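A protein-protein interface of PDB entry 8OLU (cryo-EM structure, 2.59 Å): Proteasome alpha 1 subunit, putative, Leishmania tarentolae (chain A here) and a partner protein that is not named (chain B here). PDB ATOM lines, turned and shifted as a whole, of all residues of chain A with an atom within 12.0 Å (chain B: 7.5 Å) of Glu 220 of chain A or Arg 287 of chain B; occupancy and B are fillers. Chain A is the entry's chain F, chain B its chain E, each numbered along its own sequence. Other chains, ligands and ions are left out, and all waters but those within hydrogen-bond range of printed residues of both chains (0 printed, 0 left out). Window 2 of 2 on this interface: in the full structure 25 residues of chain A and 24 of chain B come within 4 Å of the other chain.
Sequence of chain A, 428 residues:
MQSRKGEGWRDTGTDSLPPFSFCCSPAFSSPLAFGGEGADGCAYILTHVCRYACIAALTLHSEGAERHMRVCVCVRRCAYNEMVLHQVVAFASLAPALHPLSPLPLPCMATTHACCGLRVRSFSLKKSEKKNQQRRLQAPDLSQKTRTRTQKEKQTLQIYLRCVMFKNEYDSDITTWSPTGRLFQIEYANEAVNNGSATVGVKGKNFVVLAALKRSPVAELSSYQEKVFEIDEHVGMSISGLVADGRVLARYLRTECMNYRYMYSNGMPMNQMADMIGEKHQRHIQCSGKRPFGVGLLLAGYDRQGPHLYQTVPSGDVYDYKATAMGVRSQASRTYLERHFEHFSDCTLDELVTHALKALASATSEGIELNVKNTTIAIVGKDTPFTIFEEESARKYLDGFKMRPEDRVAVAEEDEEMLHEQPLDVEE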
ATOM      1  N   ARG A 215      -7.232  -8.307   4.743  1.00  0.00           N
ATOM      2  CA  ARG A 215      -6.234  -8.104   5.778  1.00  0.00           C
ATOM      3  C   ARG A 215      -4.887  -8.545   5.180  1.00  0.00           C
ATOM      4  O   ARG A 215      -4.789  -9.592   4.526  1.00  0.00           O
ATOM      5  CB  ARG A 215      -6.725  -8.792   7.061  1.00  0.00           C
ATOM      6  CG  ARG A 215      -6.034  -8.350   8.345  1.00  0.00           C
ATOM      7  CD  ARG A 215      -6.311  -9.354   9.459  1.00  0.00           C
ATOM      8  NE  ARG A 215      -5.263  -9.462  10.472  1.00  0.00           N
ATOM      9  CZ  ARG A 215      -4.995 -10.564  11.177  1.00  0.00           C
ATOM     10  NH1 ARG A 215      -5.807 -11.609  11.133  1.00  0.00           N
ATOM     11  NH2 ARG A 215      -3.891 -10.624  11.906  1.00  0.00           N
ATOM     12  N   SER A 216      -3.875  -7.671   5.371  1.00  0.00           N
ATOM     13  CA  SER A 216      -2.595  -7.699   4.665  1.00  0.00           C
ATOM     14  C   SER A 216      -1.544  -8.445   5.492  1.00  0.00           C
ATOM     15  O   SER A 216      -1.451  -8.232   6.704  1.00  0.00           O
ATOM     16  CB  SER A 216      -2.124  -6.284   4.300  1.00  0.00           C
ATOM     17  OG  SER A 216      -1.674  -5.546   5.431  1.00  0.00           O
ATOM     18  N   PRO A 217      -0.714  -9.318   4.859  1.00  0.00           N
ATOM     19  CA  PRO A 217       0.158 -10.250   5.591  1.00  0.00           C
ATOM     20  C   PRO A 217       0.902  -9.673   6.802  1.00  0.00           C
ATOM     21  O   PRO A 217       1.398  -8.548   6.758  1.00  0.00           O
ATOM     22  CB  PRO A 217       1.141 -10.721   4.499  1.00  0.00           C
ATOM     23  CG  PRO A 217       0.324 -10.681   3.220  1.00  0.00           C
ATOM     24  CD  PRO A 217      -0.590  -9.481   3.395  1.00  0.00           C
ATOM     25  N   VAL A 218       0.951 -10.467   7.887  1.00  0.00           N
ATOM     26  CA  VAL A 218       1.697 -10.144   9.097  1.00  0.00           C
ATOM     27  C   VAL A 218       3.098 -10.754   8.951  1.00  0.00           C
ATOM     28  O   VAL A 218       3.416 -11.739   9.616  1.00  0.00           O
ATOM     29  CB  VAL A 218       0.966 -10.654  10.366  1.00  0.00           C
ATOM     30  CG1 VAL A 218       1.589 -10.107  11.646  1.00  0.00           C
ATOM     31  CG2 VAL A 218      -0.533 -10.361  10.349  1.00  0.00           C
ATOM     32  N   ALA A 219       3.916 -10.159   8.063  1.00  0.00           N
ATOM     33  CA  ALA A 219       5.238 -10.648   7.677  1.00  0.00           C
ATOM     34  C   ALA A 219       5.115 -11.669   6.534  1.00  0.00           C
ATOM     35  O   ALA A 219       4.795 -11.278   5.410  1.00  0.00           O
ATOM     36  CB  ALA A 219       6.005 -11.167   8.878  1.00  0.00           C
ATOM     37  N   GLU A 220       5.374 -12.963   6.811  1.00  0.00           N
ATOM     38  CA  GLU A 220       5.257 -14.041   5.829  1.00  0.00           C
ATOM     39  C   GLU A 220       4.001 -14.885   6.098  1.00  0.00           C
ATOM     40  O   GLU A 220       3.930 -16.052   5.704  1.00  0.00           O
ATOM     41  CB  GLU A 220       6.506 -14.932   5.895  1.00  0.00           C
ATOM     42  CG  GLU A 220       7.805 -14.252   5.474  1.00  0.00           C
ATOM     43  CD  GLU A 220       8.373 -14.636   4.112  1.00  0.00           C
ATOM     44  OE1 GLU A 220       7.906 -15.638   3.523  1.00  0.00           O
ATOM     45  OE2 GLU A 220       9.295 -13.931   3.648  1.00  0.00           O
ATOM     46  N   LEU A 221       2.985 -14.261   6.720  1.00  0.00           N
ATOM     47  CA  LEU A 221       2.008 -14.954   7.551  1.00  0.00           C
ATOM     48  C   LEU A 221       0.595 -14.454   7.237  1.00  0.00           C
ATOM     49  O   LEU A 221       0.122 -13.505   7.867  1.00  0.00           O
ATOM     50  CB  LEU A 221       2.387 -14.677   9.012  1.00  0.00           C
ATOM     51  CG  LEU A 221       1.977 -15.723  10.047  1.00  0.00           C
ATOM     52  CD1 LEU A 221       2.411 -15.255  11.426  1.00  0.00           C
ATOM     53  CD2 LEU A 221       0.472 -15.996   9.995  1.00  0.00           C
ATOM     54  N   SER A 222      -0.083 -15.129   6.291  1.00  0.00           N
ATOM     55  CA  SER A 222      -1.299 -14.598   5.687  1.00  0.00           C
ATOM     56  C   SER A 222      -2.530 -14.866   6.570  1.00  0.00           C
ATOM     57  O   SER A 222      -2.453 -14.886   7.805  1.00  0.00           O
ATOM     58  CB  SER A 222      -1.462 -15.088   4.237  1.00  0.00           C
ATOM     59  OG  SER A 222      -2.130 -16.340   4.162  1.00  0.00           O
ATOM     60  N   SER A 223      -3.673 -15.059   5.902  1.00  0.00           N
ATOM     61  CA  SER A 223      -4.969 -14.836   6.510  1.00  0.00           C
ATOM     62  C   SER A 223      -5.971 -14.422   5.429  1.00  0.00           C
ATOM     63  O   SER A 223      -6.082 -13.248   5.092  1.00  0.00           O
ATOM     64  CB  SER A 223      -4.880 -13.820   7.653  1.00  0.00           C
ATOM     65  OG  SER A 223      -6.123 -13.149   7.860  1.00  0.00           O
ATOM     66  N   TYR A 224      -6.697 -15.403   4.890  1.00  0.00           N
ATOM     67  CA  TYR A 224      -7.930 -15.165   4.150  1.00  0.00           C
ATOM     68  C   TYR A 224      -9.109 -15.007   5.118  1.00  0.00           C
ATOM     69  O   TYR A 224      -9.188 -15.711   6.116  1.00  0.00           O
ATOM     70  CB  TYR A 224      -8.144 -16.336   3.188  1.00  0.00           C
ATOM     71  CG  TYR A 224      -9.321 -16.293   2.241  1.00  0.00           C
ATOM     72  CD1 TYR A 224      -9.439 -15.320   1.249  1.00  0.00           C
ATOM     73  CD2 TYR A 224     -10.267 -17.318   2.263  1.00  0.00           C
ATOM     74  CE1 TYR A 224     -10.498 -15.341   0.347  1.00  0.00           C
ATOM     75  CE2 TYR A 224     -11.331 -17.354   1.373  1.00  0.00           C
ATOM     76  CZ  TYR A 224     -11.448 -16.359   0.412  1.00  0.00           C
ATOM     77  OH  TYR A 224     -12.514 -16.424  -0.459  1.00  0.00           O
ATOM     78  N   ASN A 371      -2.263  -4.400  -3.373  1.00  0.00           N
ATOM     79  CA  ASN A 371      -1.566  -5.468  -4.064  1.00  0.00           C
ATOM     80  C   ASN A 371      -2.473  -6.693  -4.063  1.00  0.00           C
ATOM     81  O   ASN A 371      -3.520  -6.695  -3.438  1.00  0.00           O
ATOM     82  CB  ASN A 371      -0.202  -5.753  -3.422  1.00  0.00           C
ATOM     83  CG  ASN A 371      -0.313  -6.065  -1.943  1.00  0.00           C
ATOM     84  OD1 ASN A 371      -0.573  -7.206  -1.550  1.00  0.00           O
ATOM     85  ND2 ASN A 371      -0.122  -5.046  -1.121  1.00  0.00           N
ATOM     86  N   VAL A 372      -2.052  -7.746  -4.741  1.00  0.00           N
ATOM     87  CA  VAL A 372      -2.951  -8.838  -5.038  1.00  0.00           C
ATOM     88  C   VAL A 372      -3.325  -9.622  -3.785  1.00  0.00           C
ATOM     89  O   VAL A 372      -4.143 -10.535  -3.876  1.00  0.00           O
ATOM     90  CB  VAL A 372      -2.323  -9.790  -6.069  1.00  0.00           C
ATOM     91  CG1 VAL A 372      -2.485  -9.256  -7.483  1.00  0.00           C
ATOM     92  CG2 VAL A 372      -0.859 -10.094  -5.732  1.00  0.00           C
ATOM     93  N   LYS A 373      -2.703  -9.341  -2.636  1.00  0.00           N
ATOM     94  CA  LYS A 373      -2.936 -10.214  -1.496  1.00  0.00           C
ATOM     95  C   LYS A 373      -3.547  -9.432  -0.341  1.00  0.00           C
ATOM     96  O   LYS A 373      -3.726  -9.974   0.751  1.00  0.00           O
ATOM     97  CB  LYS A 373      -1.665 -10.980  -1.113  1.00  0.00           C
ATOM     98  CG  LYS A 373      -0.399 -10.154  -0.916  1.00  0.00           C
ATOM     99  CD  LYS A 373       0.861 -11.008  -0.839  1.00  0.00           C
ATOM    100  CE  LYS A 373       0.957 -12.011  -1.972  1.00  0.00           C
ATOM    101  NZ  LYS A 373       2.356 -12.418  -2.232  1.00  0.00           N
ATOM    102  N   ASN A 374      -3.911  -8.176  -0.595  1.00  0.00           N
ATOM    103  CA  ASN A 374      -4.738  -7.465   0.355  1.00  0.00           C
ATOM    104  C   ASN A 374      -5.906  -6.803  -0.370  1.00  0.00           C
ATOM    105  O   ASN A 374      -6.437  -5.814   0.122  1.00  0.00           O
ATOM    106  CB  ASN A 374      -3.920  -6.454   1.164  1.00  0.00           C
ATOM    107  CG  ASN A 374      -3.448  -5.276   0.354  1.00  0.00           C
ATOM    108  OD1 ASN A 374      -3.569  -5.280  -0.862  1.00  0.00           O
ATOM    109  ND2 ASN A 374      -2.907  -4.268   1.021  1.00  0.00           N
ATOM    110  N   GLU A 391      -5.614 -14.402  -8.730  1.00  0.00           N
ATOM    111  CA  GLU A 391      -4.311 -13.756  -8.691  1.00  0.00           C
ATOM    112  C   GLU A 391      -3.762 -13.491 -10.091  1.00  0.00           C
ATOM    113  O   GLU A 391      -2.888 -12.642 -10.245  1.00  0.00           O
ATOM    114  CB  GLU A 391      -3.356 -14.621  -7.866  1.00  0.00           C
ATOM    115  CG  GLU A 391      -3.880 -14.893  -6.462  1.00  0.00           C
ATOM    116  CD  GLU A 391      -4.390 -13.648  -5.754  1.00  0.00           C
ATOM    117  OE1 GLU A 391      -3.568 -12.951  -5.149  1.00  0.00           O
ATOM    118  OE2 GLU A 391      -5.595 -13.349  -5.863  1.00  0.00           O
ATOM    119  N   ARG A 395      -3.789  -9.136 -11.054  1.00  0.00           N
ATOM    120  CA  ARG A 395      -2.456  -8.564 -11.187  1.00  0.00           C
ATOM    121  C   ARG A 395      -2.456  -7.511 -12.296  1.00  0.00           C
ATOM    122  O   ARG A 395      -1.888  -6.429 -12.131  1.00  0.00           O
ATOM    123  CB  ARG A 395      -1.454  -9.697 -11.450  1.00  0.00           C
ATOM    124  CG  ARG A 395       0.017  -9.309 -11.327  1.00  0.00           C
ATOM    125  CD  ARG A 395       0.882 -10.544 -11.139  1.00  0.00           C
ATOM    126  NE  ARG A 395       0.649 -11.141  -9.827  1.00  0.00           N
ATOM    127  CZ  ARG A 395       1.234 -12.243  -9.373  1.00  0.00           C
ATOM    128  NH1 ARG A 395       1.864 -13.054 -10.205  1.00  0.00           N
ATOM    129  NH2 ARG A 395       1.178 -12.527  -8.083  1.00  0.00           N
ATOM    130  N   ARG B 141       0.965 -24.276   9.196  1.00  0.00           N
ATOM    131  CA  ARG B 141       0.848 -24.773   7.842  1.00  0.00           C
ATOM    132  C   ARG B 141       2.255 -24.869   7.291  1.00  0.00           C
ATOM    133  O   ARG B 141       3.066 -23.958   7.450  1.00  0.00           O
ATOM    134  CB  ARG B 141       0.038 -23.812   6.968  1.00  0.00           C
ATOM    135  CG  ARG B 141      -0.972 -24.472   6.037  1.00  0.00           C
ATOM    136  CD  ARG B 141      -0.696 -24.520   4.546  1.00  0.00           C
ATOM    137  NE  ARG B 141       0.000 -23.345   4.078  1.00  0.00           N
ATOM    138  CZ  ARG B 141       1.155 -23.402   3.437  1.00  0.00           C
ATOM    139  NH1 ARG B 141       1.362 -24.384   2.570  1.00  0.00           N
ATOM    140  NH2 ARG B 141       2.078 -22.478   3.674  1.00  0.00           N
ATOM    141  N   THR B 142       2.531 -26.007   6.669  1.00  0.00           N
ATOM    142  CA  THR B 142       3.744 -26.200   5.909  1.00  0.00           C
ATOM    143  C   THR B 142       3.318 -26.850   4.603  1.00  0.00           C
ATOM    144  O   THR B 142       2.183 -27.292   4.491  1.00  0.00           O
ATOM    145  CB  THR B 142       4.789 -26.999   6.700  1.00  0.00           C
ATOM    146  OG1 THR B 142       4.504 -28.393   6.583  1.00  0.00           O
ATOM    147  CG2 THR B 142       4.887 -26.589   8.157  1.00  0.00           C
ATOM    148  N   PRO B 143       4.159 -26.882   3.551  1.00  0.00           N
ATOM    149  CA  PRO B 143       3.770 -27.591   2.339  1.00  0.00           C
ATOM    150  C   PRO B 143       3.871 -29.100   2.527  1.00  0.00           C
ATOM    151  O   PRO B 143       3.217 -29.840   1.795  1.00  0.00           O
ATOM    152  CB  PRO B 143       4.723 -27.013   1.286  1.00  0.00           C
ATOM    153  CG  PRO B 143       5.299 -25.750   1.953  1.00  0.00           C
ATOM    154  CD  PRO B 143       5.424 -26.145   3.406  1.00  0.00           C
ATOM    155  N   ASP B 266      -1.799 -19.321   8.275  1.00  0.00           N
ATOM    156  CA  ASP B 266      -0.605 -20.086   7.957  1.00  0.00           C
ATOM    157  C   ASP B 266       0.058 -20.561   9.247  1.00  0.00           C
ATOM    158  O   ASP B 266       0.742 -21.576   9.309  1.00  0.00           O
ATOM    159  CB  ASP B 266       0.368 -19.234   7.126  1.00  0.00           C
ATOM    160  CG  ASP B 266       0.034 -19.098   5.636  1.00  0.00           C
ATOM    161  OD1 ASP B 266      -0.603 -20.039   5.058  1.00  0.00           O
ATOM    162  OD2 ASP B 266       0.389 -18.022   5.051  1.00  0.00           O
ATOM    163  N   ALA B 267      -0.103 -19.771  10.289  1.00  0.00           N
ATOM    164  CA  ALA B 267       0.295 -20.175  11.619  1.00  0.00           C
ATOM    165  C   ALA B 267      -0.578 -19.402  12.596  1.00  0.00           C
ATOM    166  O   ALA B 267      -1.005 -18.285  12.298  1.00  0.00           O
ATOM    167  CB  ALA B 267       1.747 -19.873  11.785  1.00  0.00           C
ATOM    168  N   PHE B 281       5.975 -16.389  15.799  1.00  0.00           N
ATOM    169  CA  PHE B 281       5.655 -16.743  14.423  1.00  0.00           C
ATOM    170  C   PHE B 281       6.129 -15.662  13.449  1.00  0.00           C
ATOM    171  O   PHE B 281       6.648 -15.981  12.390  1.00  0.00           O
ATOM    172  CB  PHE B 281       4.146 -16.933  14.241  1.00  0.00           C
ATOM    173  CG  PHE B 281       3.585 -18.223  14.775  1.00  0.00           C
ATOM    174  CD1 PHE B 281       4.225 -19.430  14.532  1.00  0.00           C
ATOM    175  CD2 PHE B 281       2.374 -18.237  15.447  1.00  0.00           C
ATOM    176  CE1 PHE B 281       3.685 -20.625  14.983  1.00  0.00           C
ATOM    177  CE2 PHE B 281       1.844 -19.430  15.917  1.00  0.00           C
ATOM    178  CZ  PHE B 281       2.505 -20.618  15.692  1.00  0.00           C
ATOM    179  N   THR B 282       5.918 -14.391  13.817  1.00  0.00           N
ATOM    180  CA  THR B 282       6.282 -13.216  13.029  1.00  0.00           C
ATOM    181  C   THR B 282       7.771 -13.244  12.684  1.00  0.00           C
ATOM    182  O   THR B 282       8.167 -12.750  11.628  1.00  0.00           O
ATOM    183  CB  THR B 282       5.865 -11.932  13.785  1.00  0.00           C
ATOM    184  OG1 THR B 282       4.632 -11.474  13.225  1.00  0.00           O
ATOM    185  CG2 THR B 282       6.867 -10.791  13.736  1.00  0.00           C
ATOM    186  N   GLU B 283       8.583 -13.802  13.591  1.00  0.00           N
ATOM    187  CA  GLU B 283      10.029 -13.817  13.445  1.00  0.00           C
ATOM    188  C   GLU B 283      10.486 -15.080  12.692  1.00  0.00           C
ATOM    189  O   GLU B 283      11.284 -14.962  11.756  1.00  0.00           O
ATOM    190  CB  GLU B 283      10.641 -13.630  14.838  1.00  0.00           C
ATOM    191  CG  GLU B 283      12.111 -14.005  14.938  1.00  0.00           C
ATOM    192  CD  GLU B 283      12.692 -14.023  16.346  1.00  0.00           C
ATOM    193  OE1 GLU B 283      13.851 -13.581  16.515  1.00  0.00           O
ATOM    194  OE2 GLU B 283      11.986 -14.470  17.275  1.00  0.00           O
ATOM    195  N   ARG B 284       9.973 -16.271  13.066  1.00  0.00           N
ATOM    196  CA  ARG B 284      10.578 -17.548  12.678  1.00  0.00           C
ATOM    197  C   ARG B 284       9.756 -18.342  11.663  1.00  0.00           C
ATOM    198  O   ARG B 284      10.182 -19.414  11.236  1.00  0.00           O
ATOM    199  CB  ARG B 284      10.717 -18.500  13.870  1.00  0.00           C
ATOM    200  CG  ARG B 284      11.397 -17.903  15.093  1.00  0.00           C
ATOM    201  CD  ARG B 284      12.682 -18.610  15.447  1.00  0.00           C
ATOM    202  NE  ARG B 284      12.397 -19.999  15.789  1.00  0.00           N
ATOM    203  CZ  ARG B 284      12.388 -20.495  17.021  1.00  0.00           C
ATOM    204  NH1 ARG B 284      12.340 -19.689  18.077  1.00  0.00           N
ATOM    205  NH2 ARG B 284      12.404 -21.811  17.178  1.00  0.00           N
ATOM    206  N   TYR B 285       8.567 -17.880  11.298  1.00  0.00           N
ATOM    207  CA  TYR B 285       7.746 -18.700  10.422  1.00  0.00           C
ATOM    208  C   TYR B 285       7.887 -18.181   8.998  1.00  0.00           C
ATOM    209  O   TYR B 285       7.614 -17.008   8.730  1.00  0.00           O
ATOM    210  CB  TYR B 285       6.267 -18.681  10.813  1.00  0.00           C
ATOM    211  CG  TYR B 285       5.380 -19.323   9.773  1.00  0.00           C
ATOM    212  CD1 TYR B 285       4.780 -18.588   8.757  1.00  0.00           C
ATOM    213  CD2 TYR B 285       5.144 -20.689   9.800  1.00  0.00           C
ATOM    214  CE1 TYR B 285       4.004 -19.203   7.781  1.00  0.00           C
ATOM    215  CE2 TYR B 285       4.348 -21.312   8.850  1.00  0.00           C
ATOM    216  CZ  TYR B 285       3.764 -20.573   7.840  1.00  0.00           C
ATOM    217  OH  TYR B 285       2.995 -21.275   6.919  1.00  0.00           O
ATOM    218  N   HIS B 286       8.309 -19.068   8.094  1.00  0.00           N
ATOM    219  CA  HIS B 286       8.301 -18.748   6.678  1.00  0.00           C
ATOM    220  C   HIS B 286       7.392 -19.746   5.977  1.00  0.00           C
ATOM    221  O   HIS B 286       7.216 -20.858   6.464  1.00  0.00           O
ATOM    222  CB  HIS B 286       9.724 -18.709   6.084  1.00  0.00           C
ATOM    223  CG  HIS B 286      10.582 -19.914   6.335  1.00  0.00           C
ATOM    224  ND1 HIS B 286      10.800 -20.904   5.399  1.00  0.00           N
ATOM    225  CD2 HIS B 286      11.277 -20.257   7.461  1.00  0.00           C
ATOM    226  CE1 HIS B 286      11.600 -21.831   5.926  1.00  0.00           C
ATOM    227  NE2 HIS B 286      11.912 -21.445   7.209  1.00  0.00           N
ATOM    228  N   ARG B 287       6.845 -19.336   4.826  1.00  0.00           N
ATOM    229  CA  ARG B 287       5.812 -20.094   4.135  1.00  0.00           C
ATOM    230  C   ARG B 287       6.362 -21.402   3.572  1.00  0.00           C
ATOM    231  O   ARG B 287       5.631 -22.116   2.886  1.00  0.00           O
ATOM    232  CB  ARG B 287       5.149 -19.262   3.022  1.00  0.00           C
ATOM    233  CG  ARG B 287       3.777 -18.711   3.396  1.00  0.00           C
ATOM    234  CD  ARG B 287       3.154 -17.757   2.391  1.00  0.00           C
ATOM    235  NE  ARG B 287       3.905 -16.505   2.306  1.00  0.00           N
ATOM    236  CZ  ARG B 287       4.619 -16.114   1.250  1.00  0.00           C
ATOM    237  NH1 ARG B 287       4.426 -16.671   0.064  1.00  0.00           N
ATOM    238  NH2 ARG B 287       5.523 -15.157   1.383  1.00  0.00           N
ATOM    239  N   ASN B 288       7.616 -21.750   3.881  1.00  0.00           N
ATOM    240  CA  ASN B 288       8.277 -22.763   3.077  1.00  0.00           C
ATOM    241  C   ASN B 288       9.062 -23.753   3.936  1.00  0.00           C
ATOM    242  O   ASN B 288       9.955 -24.423   3.423  1.00  0.00           O
ATOM    243  CB  ASN B 288       9.112 -22.080   1.985  1.00  0.00           C
ATOM    244  CG  ASN B 288       9.456 -23.024   0.855  1.00  0.00           C
ATOM    245  OD1 ASN B 288      10.588 -23.025   0.379  1.00  0.00           O
ATOM    246  ND2 ASN B 288       8.492 -23.824   0.422  1.00  0.00           N
ATOM    247  N   MET B 289       8.677 -23.911   5.210  1.00  0.00           N
ATOM    248  CA  MET B 289       9.414 -24.759   6.141  1.00  0.00           C
ATOM    249  C   MET B 289       9.029 -26.217   5.961  1.00  0.00           C
ATOM    250  O   MET B 289       7.994 -26.535   5.376  1.00  0.00           O
ATOM    251  CB  MET B 289       9.222 -24.391   7.624  1.00  0.00           C
ATOM    252  CG  MET B 289       7.882 -23.778   8.035  1.00  0.00           C
ATOM    253  SD  MET B 289       7.968 -22.790   9.582  1.00  0.00           S
ATOM    254  CE  MET B 289       9.340 -23.523  10.474  1.00  0.00           C
ATOM    255  N   THR B 290       9.891 -27.100   6.469  1.00  0.00           N
ATOM    256  CA  THR B 290       9.624 -28.526   6.405  1.00  0.00           C
ATOM    257  C   THR B 290       8.699 -28.871   7.558  1.00  0.00           C
ATOM    258  O   THR B 290       8.482 -28.059   8.452  1.00  0.00           O
ATOM    259  CB  THR B 290      10.907 -29.374   6.424  1.00  0.00           C
ATOM    260  OG1 THR B 290      11.587 -29.248   7.676  1.00  0.00           O
ATOM    261  CG2 THR B 290      11.856 -29.007   5.300  1.00  0.00           C
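Among the printed residues, pairs that only touch across the chains: Val 218 of chain A with Thr 282 of chain B (3.7 Å), Ala 219 of chain A with Thr 282 of chain B (3.8 Å), Glu 220 of chain A with Tyr 285 of chain B (3.7 Å), Leu 221 of chain A with Ala 267 of chain B (3.6 Å) and Leu 221 of chain A with Phe 281 of chain B (3.7 Å).
Printed residues of chain B that touch a printed residue of chain A: Asp 266, Ala 267, Phe 281, Thr 282, Tyr 285 and Arg 287.
Along chain A the printed residues that touch a printed residue of chain B span positions 218 to 222.
Among the printed residues, 7 pairs touch across the chains.
OD1 of Asp 266 of chain B is in salt-bridge range of NE of Arg 141 of chain B, at 3.5 Å.
The backbone carbonyl oxygen (O) of Asp 266 of chain B lies within hydrogen-bond range of the side-chain hydroxyl (OH) of Tyr 285 of chain B (3.3 Å).
O of Arg 141 of chain B is in hydrogen-bond range of OH of Tyr 285 of chain B (2.7 Å).
Ser 216 of chain A touches none of the printed residues of chain B.
Ala 219 of chain A touches just one residue of chain B: Thr 282.
Printed residues of chain B within 4 Å of Leu 221 of chain A: Ala 267 and Phe 281.
No residue of chain A comes within 4 Å of Thr 142 of chain B.
Asp 266 of chain B touches one residue of chain A.
Of the printed residues of chain A, Ala 267 of chain B touches Leu 221 (3.6 Å).
Of the printed residues of chain A, Phe 281 of chain B touches Leu 221.
Of chain A, only Val 218 and Ala 219 come within 4 Å of Thr 282 of chain B.
Tyr 285 of chain B touches just one residue of chain A: Glu 220.
No residue of chain A comes within 4 Å of His 286 of chain B.
No residue of chain A comes within 4 Å of Asn 288 of chain B.
Met 289 of chain B touches none of the printed residues of chain A.
Thr 290 of chain B touches none of the printed residues of chain A.
The nearest residue of chain B that does not touch Glu 220 of chain A is Asp 266 of chain B (4.1 Å).
The side-chain hydroxyl (OG) of Ser 222 of chain A is in hydrogen-bond range of the side-chain carboxylate (OD2) of Asp 266 of chain B, at 3.2 Å.
OE1 of Glu 220 of chain A is in salt-bridge range of NH2 of Arg 287 of chain B (3.2 Å).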
